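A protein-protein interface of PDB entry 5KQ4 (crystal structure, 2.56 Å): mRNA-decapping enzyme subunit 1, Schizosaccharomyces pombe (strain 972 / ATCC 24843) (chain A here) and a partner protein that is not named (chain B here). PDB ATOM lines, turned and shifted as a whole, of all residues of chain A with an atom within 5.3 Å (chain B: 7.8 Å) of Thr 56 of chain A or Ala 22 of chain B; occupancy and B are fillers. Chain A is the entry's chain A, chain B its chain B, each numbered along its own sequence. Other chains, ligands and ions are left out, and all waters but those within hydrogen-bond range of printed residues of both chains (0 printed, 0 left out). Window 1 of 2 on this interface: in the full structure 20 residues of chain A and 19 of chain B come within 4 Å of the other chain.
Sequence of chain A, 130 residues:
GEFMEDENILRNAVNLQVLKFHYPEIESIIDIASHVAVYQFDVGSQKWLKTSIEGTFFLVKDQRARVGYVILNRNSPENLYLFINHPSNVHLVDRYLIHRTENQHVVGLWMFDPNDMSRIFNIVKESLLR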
ATOM      1  N   VAL A  14       4.826  15.007   7.299  1.00  0.00           N
ATOM      2  CA  VAL A  14       3.543  14.514   7.793  1.00  0.00           C
ATOM      3  C   VAL A  14       3.689  13.114   8.377  1.00  0.00           C
ATOM      4  O   VAL A  14       3.137  12.815   9.443  1.00  0.00           O
ATOM      5  CB  VAL A  14       2.491  14.560   6.669  1.00  0.00           C
ATOM      6  CG1 VAL A  14       1.258  13.755   7.054  1.00  0.00           C
ATOM      7  CG2 VAL A  14       2.111  16.003   6.352  1.00  0.00           C
ATOM      8  N   ASN A  15       4.434  12.238   7.694  1.00  0.00           N
ATOM      9  CA  ASN A  15       4.618  10.873   8.184  1.00  0.00           C
ATOM     10  C   ASN A  15       5.217  10.865   9.586  1.00  0.00           C
ATOM     11  O   ASN A  15       4.705  10.194  10.490  1.00  0.00           O
ATOM     12  CB  ASN A  15       5.497  10.084   7.217  1.00  0.00           C
ATOM     13  CG  ASN A  15       4.724   9.540   6.028  1.00  0.00           C
ATOM     14  OD1 ASN A  15       3.504   9.399   6.072  1.00  0.00           O
ATOM     15  ND2 ASN A  15       5.443   9.223   4.957  1.00  0.00           N
ATOM     16  N   VAL A  18       2.820  12.073  12.132  1.00  0.00           N
ATOM     17  CA  VAL A  18       1.783  11.106  12.482  1.00  0.00           C
ATOM     18  C   VAL A  18       2.330  10.061  13.447  1.00  0.00           C
ATOM     19  O   VAL A  18       1.702   9.743  14.465  1.00  0.00           O
ATOM     20  CB  VAL A  18       1.206  10.458  11.210  1.00  0.00           C
ATOM     21  CG1 VAL A  18       0.356   9.247  11.570  1.00  0.00           C
ATOM     22  CG2 VAL A  18       0.391  11.478  10.424  1.00  0.00           C
ATOM     23  N   ALA A  33       8.045   1.225   3.611  1.00  0.00           N
ATOM     24  CA  ALA A  33       7.531   0.227   2.681  1.00  0.00           C
ATOM     25  C   ALA A  33       6.060   0.527   2.428  1.00  0.00           C
ATOM     26  O   ALA A  33       5.305   0.764   3.377  1.00  0.00           O
ATOM     27  CB  ALA A  33       7.702  -1.191   3.225  1.00  0.00           C
ATOM     28  N   SER A  34       5.660   0.522   1.151  1.00  0.00           N
ATOM     29  CA  SER A  34       4.334   1.012   0.771  1.00  0.00           C
ATOM     30  C   SER A  34       3.205   0.196   1.398  1.00  0.00           C
ATOM     31  O   SER A  34       2.216   0.763   1.881  1.00  0.00           O
ATOM     32  CB  SER A  34       4.203   1.015  -0.751  1.00  0.00           C
ATOM     33  OG  SER A  34       5.136   1.900  -1.340  1.00  0.00           O
ATOM     34  N   HIS A  35       3.330  -1.130   1.410  1.00  0.00           N
ATOM     35  CA  HIS A  35       2.273  -1.985   1.935  1.00  0.00           C
ATOM     36  C   HIS A  35       2.870  -3.290   2.436  1.00  0.00           C
ATOM     37  O   HIS A  35       3.622  -3.946   1.710  1.00  0.00           O
ATOM     38  CB  HIS A  35       1.217  -2.266   0.862  1.00  0.00           C
ATOM     39  CG  HIS A  35       0.010  -2.992   1.373  1.00  0.00           C
ATOM     40  ND1 HIS A  35      -0.973  -2.374   2.117  1.00  0.00           N
ATOM     41  CD2 HIS A  35      -0.371  -4.284   1.248  1.00  0.00           C
ATOM     42  CE1 HIS A  35      -1.909  -3.255   2.427  1.00  0.00           C
ATOM     43  NE2 HIS A  35      -1.567  -4.422   1.911  1.00  0.00           N
ATOM     44  N   VAL A  36       2.532  -3.661   3.674  1.00  0.00           N
ATOM     45  CA  VAL A  36       2.986  -4.915   4.268  1.00  0.00           C
ATOM     46  C   VAL A  36       1.828  -5.606   4.979  1.00  0.00           C
ATOM     47  O   VAL A  36       0.951  -4.951   5.548  1.00  0.00           O
ATOM     48  CB  VAL A  36       4.169  -4.699   5.238  1.00  0.00           C
ATOM     49  CG1 VAL A  36       5.302  -3.974   4.543  1.00  0.00           C
ATOM     50  CG2 VAL A  36       3.725  -3.910   6.454  1.00  0.00           C
ATOM     51  N   GLU A  54      -2.468  -4.602   8.465  1.00  0.00           N
ATOM     52  CA  GLU A  54      -2.063  -4.390   7.082  1.00  0.00           C
ATOM     53  C   GLU A  54      -1.953  -2.896   6.819  1.00  0.00           C
ATOM     54  O   GLU A  54      -2.842  -2.130   7.202  1.00  0.00           O
ATOM     55  CB  GLU A  54      -3.074  -5.026   6.123  1.00  0.00           C
ATOM     56  CG  GLU A  54      -2.482  -5.973   5.106  1.00  0.00           C
ATOM     57  CD  GLU A  54      -3.548  -6.606   4.241  1.00  0.00           C
ATOM     58  OE1 GLU A  54      -4.709  -6.693   4.693  1.00  0.00           O
ATOM     59  OE2 GLU A  54      -3.229  -7.001   3.106  1.00  0.00           O
ATOM     60  N   GLY A  55      -0.868  -2.485   6.177  1.00  0.00           N
ATOM     61  CA  GLY A  55      -0.745  -1.091   5.797  1.00  0.00           C
ATOM     62  C   GLY A  55       0.701  -0.723   5.524  1.00  0.00           C
ATOM     63  O   GLY A  55       1.527  -1.576   5.204  1.00  0.00           O
ATOM     64  N   THR A  56       0.973   0.573   5.665  1.00  0.00           N
ATOM     65  CA  THR A  56       2.288   1.127   5.384  1.00  0.00           C
ATOM     66  C   THR A  56       3.269   0.800   6.505  1.00  0.00           C
ATOM     67  O   THR A  56       2.912   0.801   7.687  1.00  0.00           O
ATOM     68  CB  THR A  56       2.191   2.640   5.200  1.00  0.00           C
ATOM     69  OG1 THR A  56       1.759   3.239   6.427  1.00  0.00           O
ATOM     70  CG2 THR A  56       1.183   2.979   4.111  1.00  0.00           C
ATOM     71  N   PHE A  57       4.511   0.522   6.122  1.00  0.00           N
ATOM     72  CA  PHE A  57       5.563   0.069   7.024  1.00  0.00           C
ATOM     73  C   PHE A  57       6.565   1.204   7.198  1.00  0.00           C
ATOM     74  O   PHE A  57       7.108   1.710   6.212  1.00  0.00           O
ATOM     75  CB  PHE A  57       6.228  -1.184   6.444  1.00  0.00           C
ATOM     76  CG  PHE A  57       7.440  -1.680   7.202  1.00  0.00           C
ATOM     77  CD1 PHE A  57       8.684  -1.080   7.061  1.00  0.00           C
ATOM     78  CD2 PHE A  57       7.333  -2.792   8.019  1.00  0.00           C
ATOM     79  CE1 PHE A  57       9.787  -1.559   7.753  1.00  0.00           C
ATOM     80  CE2 PHE A  57       8.431  -3.278   8.710  1.00  0.00           C
ATOM     81  CZ  PHE A  57       9.661  -2.660   8.573  1.00  0.00           C
ATOM     82  N   PHE A  58       6.800   1.606   8.445  1.00  0.00           N
ATOM     83  CA  PHE A  58       7.765   2.653   8.760  1.00  0.00           C
ATOM     84  C   PHE A  58       8.870   2.044   9.604  1.00  0.00           C
ATOM     85  O   PHE A  58       8.607   1.520  10.690  1.00  0.00           O
ATOM     86  CB  PHE A  58       7.134   3.821   9.523  1.00  0.00           C
ATOM     87  CG  PHE A  58       5.993   4.467   8.819  1.00  0.00           C
ATOM     88  CD1 PHE A  58       4.711   3.966   8.949  1.00  0.00           C
ATOM     89  CD2 PHE A  58       6.199   5.581   8.024  1.00  0.00           C
ATOM     90  CE1 PHE A  58       3.654   4.568   8.311  1.00  0.00           C
ATOM     91  CE2 PHE A  58       5.143   6.189   7.375  1.00  0.00           C
ATOM     92  CZ  PHE A  58       3.868   5.680   7.519  1.00  0.00           C
ATOM     93  N   VAL A  70       6.982   0.554  12.746  1.00  0.00           N
ATOM     94  CA  VAL A  70       5.565   0.807  12.968  1.00  0.00           C
ATOM     95  C   VAL A  70       4.817   0.438  11.696  1.00  0.00           C
ATOM     96  O   VAL A  70       5.267   0.751  10.587  1.00  0.00           O
ATOM     97  CB  VAL A  70       5.303   2.277  13.353  1.00  0.00           C
ATOM     98  CG1 VAL A  70       3.811   2.535  13.511  1.00  0.00           C
ATOM     99  CG2 VAL A  70       6.046   2.636  14.626  1.00  0.00           C
ATOM    100  N   ILE A  71       3.677  -0.226  11.853  1.00  0.00           N
ATOM    101  CA  ILE A  71       2.771  -0.508  10.749  1.00  0.00           C
ATOM    102  C   ILE A  71       1.441   0.157  11.072  1.00  0.00           C
ATOM    103  O   ILE A  71       0.762  -0.234  12.028  1.00  0.00           O
ATOM    104  CB  ILE A  71       2.617  -2.015  10.518  1.00  0.00           C
ATOM    105  CG1 ILE A  71       4.006  -2.638  10.338  1.00  0.00           C
ATOM    106  CG2 ILE A  71       1.734  -2.279   9.308  1.00  0.00           C
ATOM    107  CD1 ILE A  71       4.005  -4.089  10.000  1.00  0.00           C
ATOM    108  N   LEU A  72       1.066   1.153  10.273  1.00  0.00           N
ATOM    109  CA  LEU A  72      -0.203   1.848  10.449  1.00  0.00           C
ATOM    110  C   LEU A  72      -1.297   1.009   9.804  1.00  0.00           C
ATOM    111  O   LEU A  72      -1.379   0.915   8.574  1.00  0.00           O
ATOM    112  CB  LEU A  72      -0.146   3.248   9.843  1.00  0.00           C
ATOM    113  CG  LEU A  72       0.704   4.293  10.576  1.00  0.00           C
ATOM    114  CD1 LEU A  72       0.651   5.632   9.853  1.00  0.00           C
ATOM    115  CD2 LEU A  72       0.260   4.443  12.025  1.00  0.00           C
ATOM    116  N   ARG A  74      -4.514  -0.407   8.167  1.00  0.00           N
ATOM    117  CA  ARG A  74      -5.580   0.116   7.326  1.00  0.00           C
ATOM    118  C   ARG A  74      -6.939  -0.495   7.641  1.00  0.00           C
ATOM    119  O   ARG A  74      -7.954   0.021   7.161  1.00  0.00           O
ATOM    120  CB  ARG A  74      -5.261  -0.137   5.848  1.00  0.00           C
ATOM    121  CG  ARG A  74      -4.073   0.633   5.290  1.00  0.00           C
ATOM    122  CD  ARG A  74      -3.787   0.191   3.862  1.00  0.00           C
ATOM    123  NE  ARG A  74      -2.579   0.797   3.311  1.00  0.00           N
ATOM    124  CZ  ARG A  74      -2.580   1.818   2.460  1.00  0.00           C
ATOM    125  NH1 ARG A  74      -3.728   2.347   2.062  1.00  0.00           N
ATOM    126  NH2 ARG A  74      -1.436   2.309   2.002  1.00  0.00           N
ATOM    127  N   VAL B  16      -6.285  14.164  12.755  1.00  0.00           N
ATOM    128  CA  VAL B  16      -7.014  13.067  12.121  1.00  0.00           C
ATOM    129  C   VAL B  16      -6.729  13.046  10.626  1.00  0.00           C
ATOM    130  O   VAL B  16      -6.464  11.991  10.038  1.00  0.00           O
ATOM    131  CB  VAL B  16      -8.522  13.194  12.405  1.00  0.00           C
ATOM    132  CG1 VAL B  16      -9.301  12.136  11.630  1.00  0.00           C
ATOM    133  CG2 VAL B  16      -8.796  13.087  13.897  1.00  0.00           C
ATOM    134  N   LEU B  17      -6.776  14.220   9.990  1.00  0.00           N
ATOM    135  CA  LEU B  17      -6.457  14.307   8.569  1.00  0.00           C
ATOM    136  C   LEU B  17      -4.996  13.958   8.308  1.00  0.00           C
ATOM    137  O   LEU B  17      -4.677  13.335   7.289  1.00  0.00           O
ATOM    138  CB  LEU B  17      -6.789  15.702   8.038  1.00  0.00           C
ATOM    139  CG  LEU B  17      -8.272  16.085   8.059  1.00  0.00           C
ATOM    140  CD1 LEU B  17      -8.535  17.290   7.168  1.00  0.00           C
ATOM    141  CD2 LEU B  17      -9.147  14.910   7.647  1.00  0.00           C
ATOM    142  N   ASP B  18      -4.095  14.349   9.214  1.00  0.00           N
ATOM    143  CA  ASP B  18      -2.704  13.915   9.107  1.00  0.00           C
ATOM    144  C   ASP B  18      -2.617  12.398   9.059  1.00  0.00           C
ATOM    145  O   ASP B  18      -1.936  11.823   8.201  1.00  0.00           O
ATOM    146  CB  ASP B  18      -1.881  14.441  10.285  1.00  0.00           C
ATOM    147  CG  ASP B  18      -1.524  15.902  10.149  1.00  0.00           C
ATOM    148  OD1 ASP B  18      -1.723  16.471   9.058  1.00  0.00           O
ATOM    149  OD2 ASP B  18      -1.025  16.478  11.139  1.00  0.00           O
ATOM    150  N   ASP B  19      -3.309  11.735   9.987  1.00  0.00           N
ATOM    151  CA  ASP B  19      -3.260  10.281  10.073  1.00  0.00           C
ATOM    152  C   ASP B  19      -3.774   9.640   8.794  1.00  0.00           C
ATOM    153  O   ASP B  19      -3.088   8.813   8.184  1.00  0.00           O
ATOM    154  CB  ASP B  19      -4.073   9.807  11.279  1.00  0.00           C
ATOM    155  CG  ASP B  19      -3.994   8.305  11.488  1.00  0.00           C
ATOM    156  OD1 ASP B  19      -4.333   7.535  10.564  1.00  0.00           O
ATOM    157  OD2 ASP B  19      -3.592   7.887  12.591  1.00  0.00           O
ATOM    158  N   LEU B  20      -4.992  10.004   8.381  1.00  0.00           N
ATOM    159  CA  LEU B  20      -5.611   9.369   7.221  1.00  0.00           C
ATOM    160  C   LEU B  20      -4.741   9.514   5.982  1.00  0.00           C
ATOM    161  O   LEU B  20      -4.709   8.623   5.125  1.00  0.00           O
ATOM    162  CB  LEU B  20      -7.001   9.959   6.976  1.00  0.00           C
ATOM    163  CG  LEU B  20      -8.010   9.767   8.113  1.00  0.00           C
ATOM    164  CD1 LEU B  20      -9.337  10.426   7.782  1.00  0.00           C
ATOM    165  CD2 LEU B  20      -8.208   8.288   8.403  1.00  0.00           C
ATOM    166  N   SER B  21      -4.018  10.630   5.878  1.00  0.00           N
ATOM    167  CA  SER B  21      -3.112  10.834   4.754  1.00  0.00           C
ATOM    168  C   SER B  21      -1.980   9.815   4.783  1.00  0.00           C
ATOM    169  O   SER B  21      -1.769   9.072   3.818  1.00  0.00           O
ATOM    170  CB  SER B  21      -2.561  12.259   4.787  1.00  0.00           C
ATOM    171  OG  SER B  21      -3.610  13.203   4.901  1.00  0.00           O
ATOM    172  N   ALA B  22      -1.243   9.761   5.896  1.00  0.00           N
ATOM    173  CA  ALA B  22      -0.167   8.784   6.023  1.00  0.00           C
ATOM    174  C   ALA B  22      -0.695   7.356   5.970  1.00  0.00           C
ATOM    175  O   ALA B  22       0.014   6.449   5.520  1.00  0.00           O
ATOM    176  CB  ALA B  22       0.604   9.018   7.321  1.00  0.00           C
ATOM    177  N   ARG B  23      -1.938   7.140   6.400  1.00  0.00           N
ATOM    178  CA  ARG B  23      -2.480   5.788   6.480  1.00  0.00           C
ATOM    179  C   ARG B  23      -2.962   5.262   5.132  1.00  0.00           C
ATOM    180  O   ARG B  23      -2.979   4.041   4.924  1.00  0.00           O
ATOM    181  CB  ARG B  23      -3.627   5.757   7.489  1.00  0.00           C
ATOM    182  CG  ARG B  23      -3.754   4.457   8.263  1.00  0.00           C
ATOM    183  CD  ARG B  23      -4.806   4.577   9.356  1.00  0.00           C
ATOM    184  NE  ARG B  23      -4.706   3.522  10.366  1.00  0.00           N
ATOM    185  CZ  ARG B  23      -4.095   3.658  11.539  1.00  0.00           C
ATOM    186  NH1 ARG B  23      -3.523   4.810  11.856  1.00  0.00           N
ATOM    187  NH2 ARG B  23      -4.055   2.644  12.394  1.00  0.00           N
ATOM    188  N   PHE B  24      -3.362   6.141   4.212  1.00  0.00           N
ATOM    189  CA  PHE B  24      -4.079   5.691   3.025  1.00  0.00           C
ATOM    190  C   PHE B  24      -3.545   6.266   1.718  1.00  0.00           C
ATOM    191  O   PHE B  24      -3.563   5.590   0.685  1.00  0.00           O
ATOM    192  CB  PHE B  24      -5.569   6.037   3.151  1.00  0.00           C
ATOM    193  CG  PHE B  24      -6.312   5.164   4.129  1.00  0.00           C
ATOM    194  CD1 PHE B  24      -6.692   3.881   3.778  1.00  0.00           C
ATOM    195  CD2 PHE B  24      -6.651   5.633   5.388  1.00  0.00           C
ATOM    196  CE1 PHE B  24      -7.375   3.078   4.662  1.00  0.00           C
ATOM    197  CE2 PHE B  24      -7.337   4.836   6.280  1.00  0.00           C
ATOM    198  CZ  PHE B  24      -7.701   3.555   5.915  1.00  0.00           C
ATOM    199  N   ILE B  25      -3.063   7.503   1.734  1.00  0.00           N
ATOM    200  CA  ILE B  25      -2.811   8.276   0.511  1.00  0.00           C
ATOM    201  C   ILE B  25      -1.306   8.390   0.223  1.00  0.00           C
ATOM    202  O   ILE B  25      -0.839   7.990  -0.837  1.00  0.00           O
ATOM    203  CB  ILE B  25      -3.471   9.673   0.591  1.00  0.00           C
ATOM    204  CG1 ILE B  25      -4.926   9.539   1.030  1.00  0.00           C
ATOM    205  CG2 ILE B  25      -3.422  10.368  -0.751  1.00  0.00           C
ATOM    206  CD1 ILE B  25      -5.806   8.732   0.087  1.00  0.00           C
ATOM    207  N   LEU B  26      -0.533   8.942   1.165  1.00  0.00           N
ATOM    208  CA  LEU B  26       0.794   9.463   0.822  1.00  0.00           C
ATOM    209  C   LEU B  26       1.773   8.354   0.456  1.00  0.00           C
ATOM    210  O   LEU B  26       2.617   8.542  -0.423  1.00  0.00           O
ATOM    211  CB  LEU B  26       1.333  10.295   1.987  1.00  0.00           C
ATOM    212  CG  LEU B  26       0.428  11.454   2.408  1.00  0.00           C
ATOM    213  CD1 LEU B  26       1.055  12.310   3.506  1.00  0.00           C
ATOM    214  CD2 LEU B  26       0.032  12.308   1.211  1.00  0.00           C
ATOM    215  N   ASN B  27       1.687   7.201   1.122  1.00  0.00           N
ATOM    216  CA  ASN B  27       2.648   6.109   0.951  1.00  0.00           C
ATOM    217  C   ASN B  27       1.963   4.966   0.204  1.00  0.00           C
ATOM    218  O   ASN B  27       1.480   4.001   0.798  1.00  0.00           O
ATOM    219  CB  ASN B  27       3.195   5.659   2.306  1.00  0.00           C
ATOM    220  CG  ASN B  27       3.670   6.820   3.150  1.00  0.00           C
ATOM    221  OD1 ASN B  27       4.786   7.312   2.978  1.00  0.00           O
ATOM    222  ND2 ASN B  27       2.815   7.280   4.059  1.00  0.00           N
ATOM    223  N   LEU B  28       1.914   5.097  -1.115  1.00  0.00           N
ATOM    224  CA  LEU B  28       1.420   4.080  -2.025  1.00  0.00           C
ATOM    225  C   LEU B  28       2.513   3.745  -3.027  1.00  0.00           C
ATOM    226  O   LEU B  28       3.399   4.568  -3.290  1.00  0.00           O
ATOM    227  CB  LEU B  28       0.162   4.559  -2.767  1.00  0.00           C
ATOM    228  CG  LEU B  28      -1.073   4.762  -1.888  1.00  0.00           C
ATOM    229  CD1 LEU B  28      -2.170   5.486  -2.642  1.00  0.00           C
ATOM    230  CD2 LEU B  28      -1.582   3.429  -1.363  1.00  0.00           C
ATOM    231  N   PRO B  29       2.498   2.540  -3.590  1.00  0.00           N
ATOM    232  CA  PRO B  29       3.450   2.218  -4.657  1.00  0.00           C
ATOM    233  C   PRO B  29       3.306   3.189  -5.818  1.00  0.00           C
ATOM    234  O   PRO B  29       2.219   3.699  -6.092  1.00  0.00           O
ATOM    235  CB  PRO B  29       3.061   0.791  -5.065  1.00  0.00           C
ATOM    236  CG  PRO B  29       2.330   0.237  -3.877  1.00  0.00           C
ATOM    237  CD  PRO B  29       1.626   1.403  -3.255  1.00  0.00           C
ATOM    238  N   LEU B  73     -10.050  16.785   2.895  1.00  0.00           N
ATOM    239  CA  LEU B  73      -8.765  16.111   2.734  1.00  0.00           C
ATOM    240  C   LEU B  73      -7.901  16.816   1.696  1.00  0.00           C
ATOM    241  O   LEU B  73      -6.675  16.889   1.845  1.00  0.00           O
ATOM    242  CB  LEU B  73      -8.981  14.647   2.345  1.00  0.00           C
ATOM    243  CG  LEU B  73      -7.858  13.646   2.641  1.00  0.00           C
ATOM    244  CD1 LEU B  73      -7.716  13.434   4.138  1.00  0.00           C
ATOM    245  CD2 LEU B  73      -8.122  12.326   1.933  1.00  0.00           C
ATOM    246  N   CYS B  77      -4.232  18.494   2.420  1.00  0.00           N
ATOM    247  CA  CYS B  77      -3.089  17.842   1.789  1.00  0.00           C
ATOM    248  C   CYS B  77      -2.821  18.485   0.434  1.00  0.00           C
ATOM    249  O   CYS B  77      -3.412  18.083  -0.579  1.00  0.00           O
ATOM    250  CB  CYS B  77      -3.345  16.341   1.634  1.00  0.00           C
ATOM    251  SG  CYS B  77      -1.916  15.395   1.048  1.00  0.00           S
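CG1 of Val 14 of chain A touches O of Asp 18 of chain B, 3.9 Å away.
CD1 of Leu 26 of chain B touches CG1 of Val 14 of chain A, 3.8 Å away.
Val 18 of chain A touches Asp 19 of chain B (CG2 to N, 3.7 Å).
CG2 of Val 18 of chain A touches CB of Ala 22 of chain B, 3.97 Å away.
Ser 34 of chain A touches Pro 29 of chain B (OG to N, 3.5 Å).
Ala 22 of chain B touches Thr 56 of chain A.
ND2 of Asn 27 of chain B touches CZ of Phe 58 of chain A, at 3.95 Å.
Leu 72 of chain A touches Arg 23 of chain B.
Asn 27 of chain B touches Arg 74 of chain A.
CD2 of Leu 28 of chain B touches NH2 of Arg 74 of chain A, 3.5 Å away.
O of Glu 54 of chain A lies within hydrogen-bond range of N of Arg 74 of chain A (2.6 Å).
The backbone carbonyl oxygen (O) of Thr 56 of chain A sits at hydrogen-bond distance from the backbone NH (N) of Leu 72 of chain A (3.2 Å).
O of Val 70 of chain A lies within hydrogen-bond range of N of Phe 58 of chain A (2.8 Å).
The side-chain carboxylate of Asp 19 of chain B lies within salt-bridge range of the guanidinium group of Arg 23 of chain B (3.1 Å).
O of Ser 21 of chain B is in hydrogen-bond range of N of Leu 26 of chain B.
The side-chain amide nitrogen (ND2) of Asn 27 of chain B sits at hydrogen-bond distance from the backbone carbonyl oxygen (O) of Ala 22 of chain B, 3.3 Å away.
ND2 of Asn 15 of chain A sits at hydrogen-bond distance from OD1 of Asn 27 of chain B (2.8 Å).
NH1 of Arg 74 of chain A sits close to O of Arg 23 of chain B.
The backbone carbonyl oxygen (O) of Asn 27 of chain B lies close to the backbone carbonyl oxygen (O) of Ser 34 of chain A, 3.5 Å away.
Thr 56 of chain A touches just these residues of chain B: Ala 22 and Asn 27.
Printed residues of chain A within 4 Å of Ala 22 of chain B: Asn 15, Val 18 and Thr 56.
No residue of chain B comes within 4 Å of Gly 55 of chain A.
Of the printed residues of chain A, Arg 23 of chain B touches Leu 72 (3.8 Å) and Arg 74 (3.3 Å).
Of the printed residues of chain A, Leu 26 of chain B touches Val 14.
Of the printed residues of chain A, Leu 28 of chain B touches Ser 34 (3.6 Å) and Arg 74 (3.5 Å).
Printed residues of chain B within 4 Å of Arg 74 of chain A: Arg 23, Phe 24, Asn 27 and Leu 28.
Leu 20 of chain B touches none of the printed residues of chain A.
Leu 73 of chain B touches none of the printed residues of chain A.
Of the 16 printed residues of chain B, 9 touch a printed residue of chain A.
Printed residues of chain B that touch a printed residue of chain A: Asp 18, Asp 19, Ala 22, Arg 23, Phe 24, Leu 26, Asn 27, Leu 28 and Pro 29.
Hydrophobic or aromatic side chains of chain B within 4 Å of the printed part of chain A: Ala 22, Phe 24, Leu 26, Leu 28 and Pro 29.
Hydrophobic or aromatic side chains of chain A that line the printed part of chain B: Val 14, Val 18, Phe 58 and Leu 72.
Among the printed residues, no Asp or Glu carboxylate lies within 4 Å of a Lys or Arg side-chain nitrogen of the other chain.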
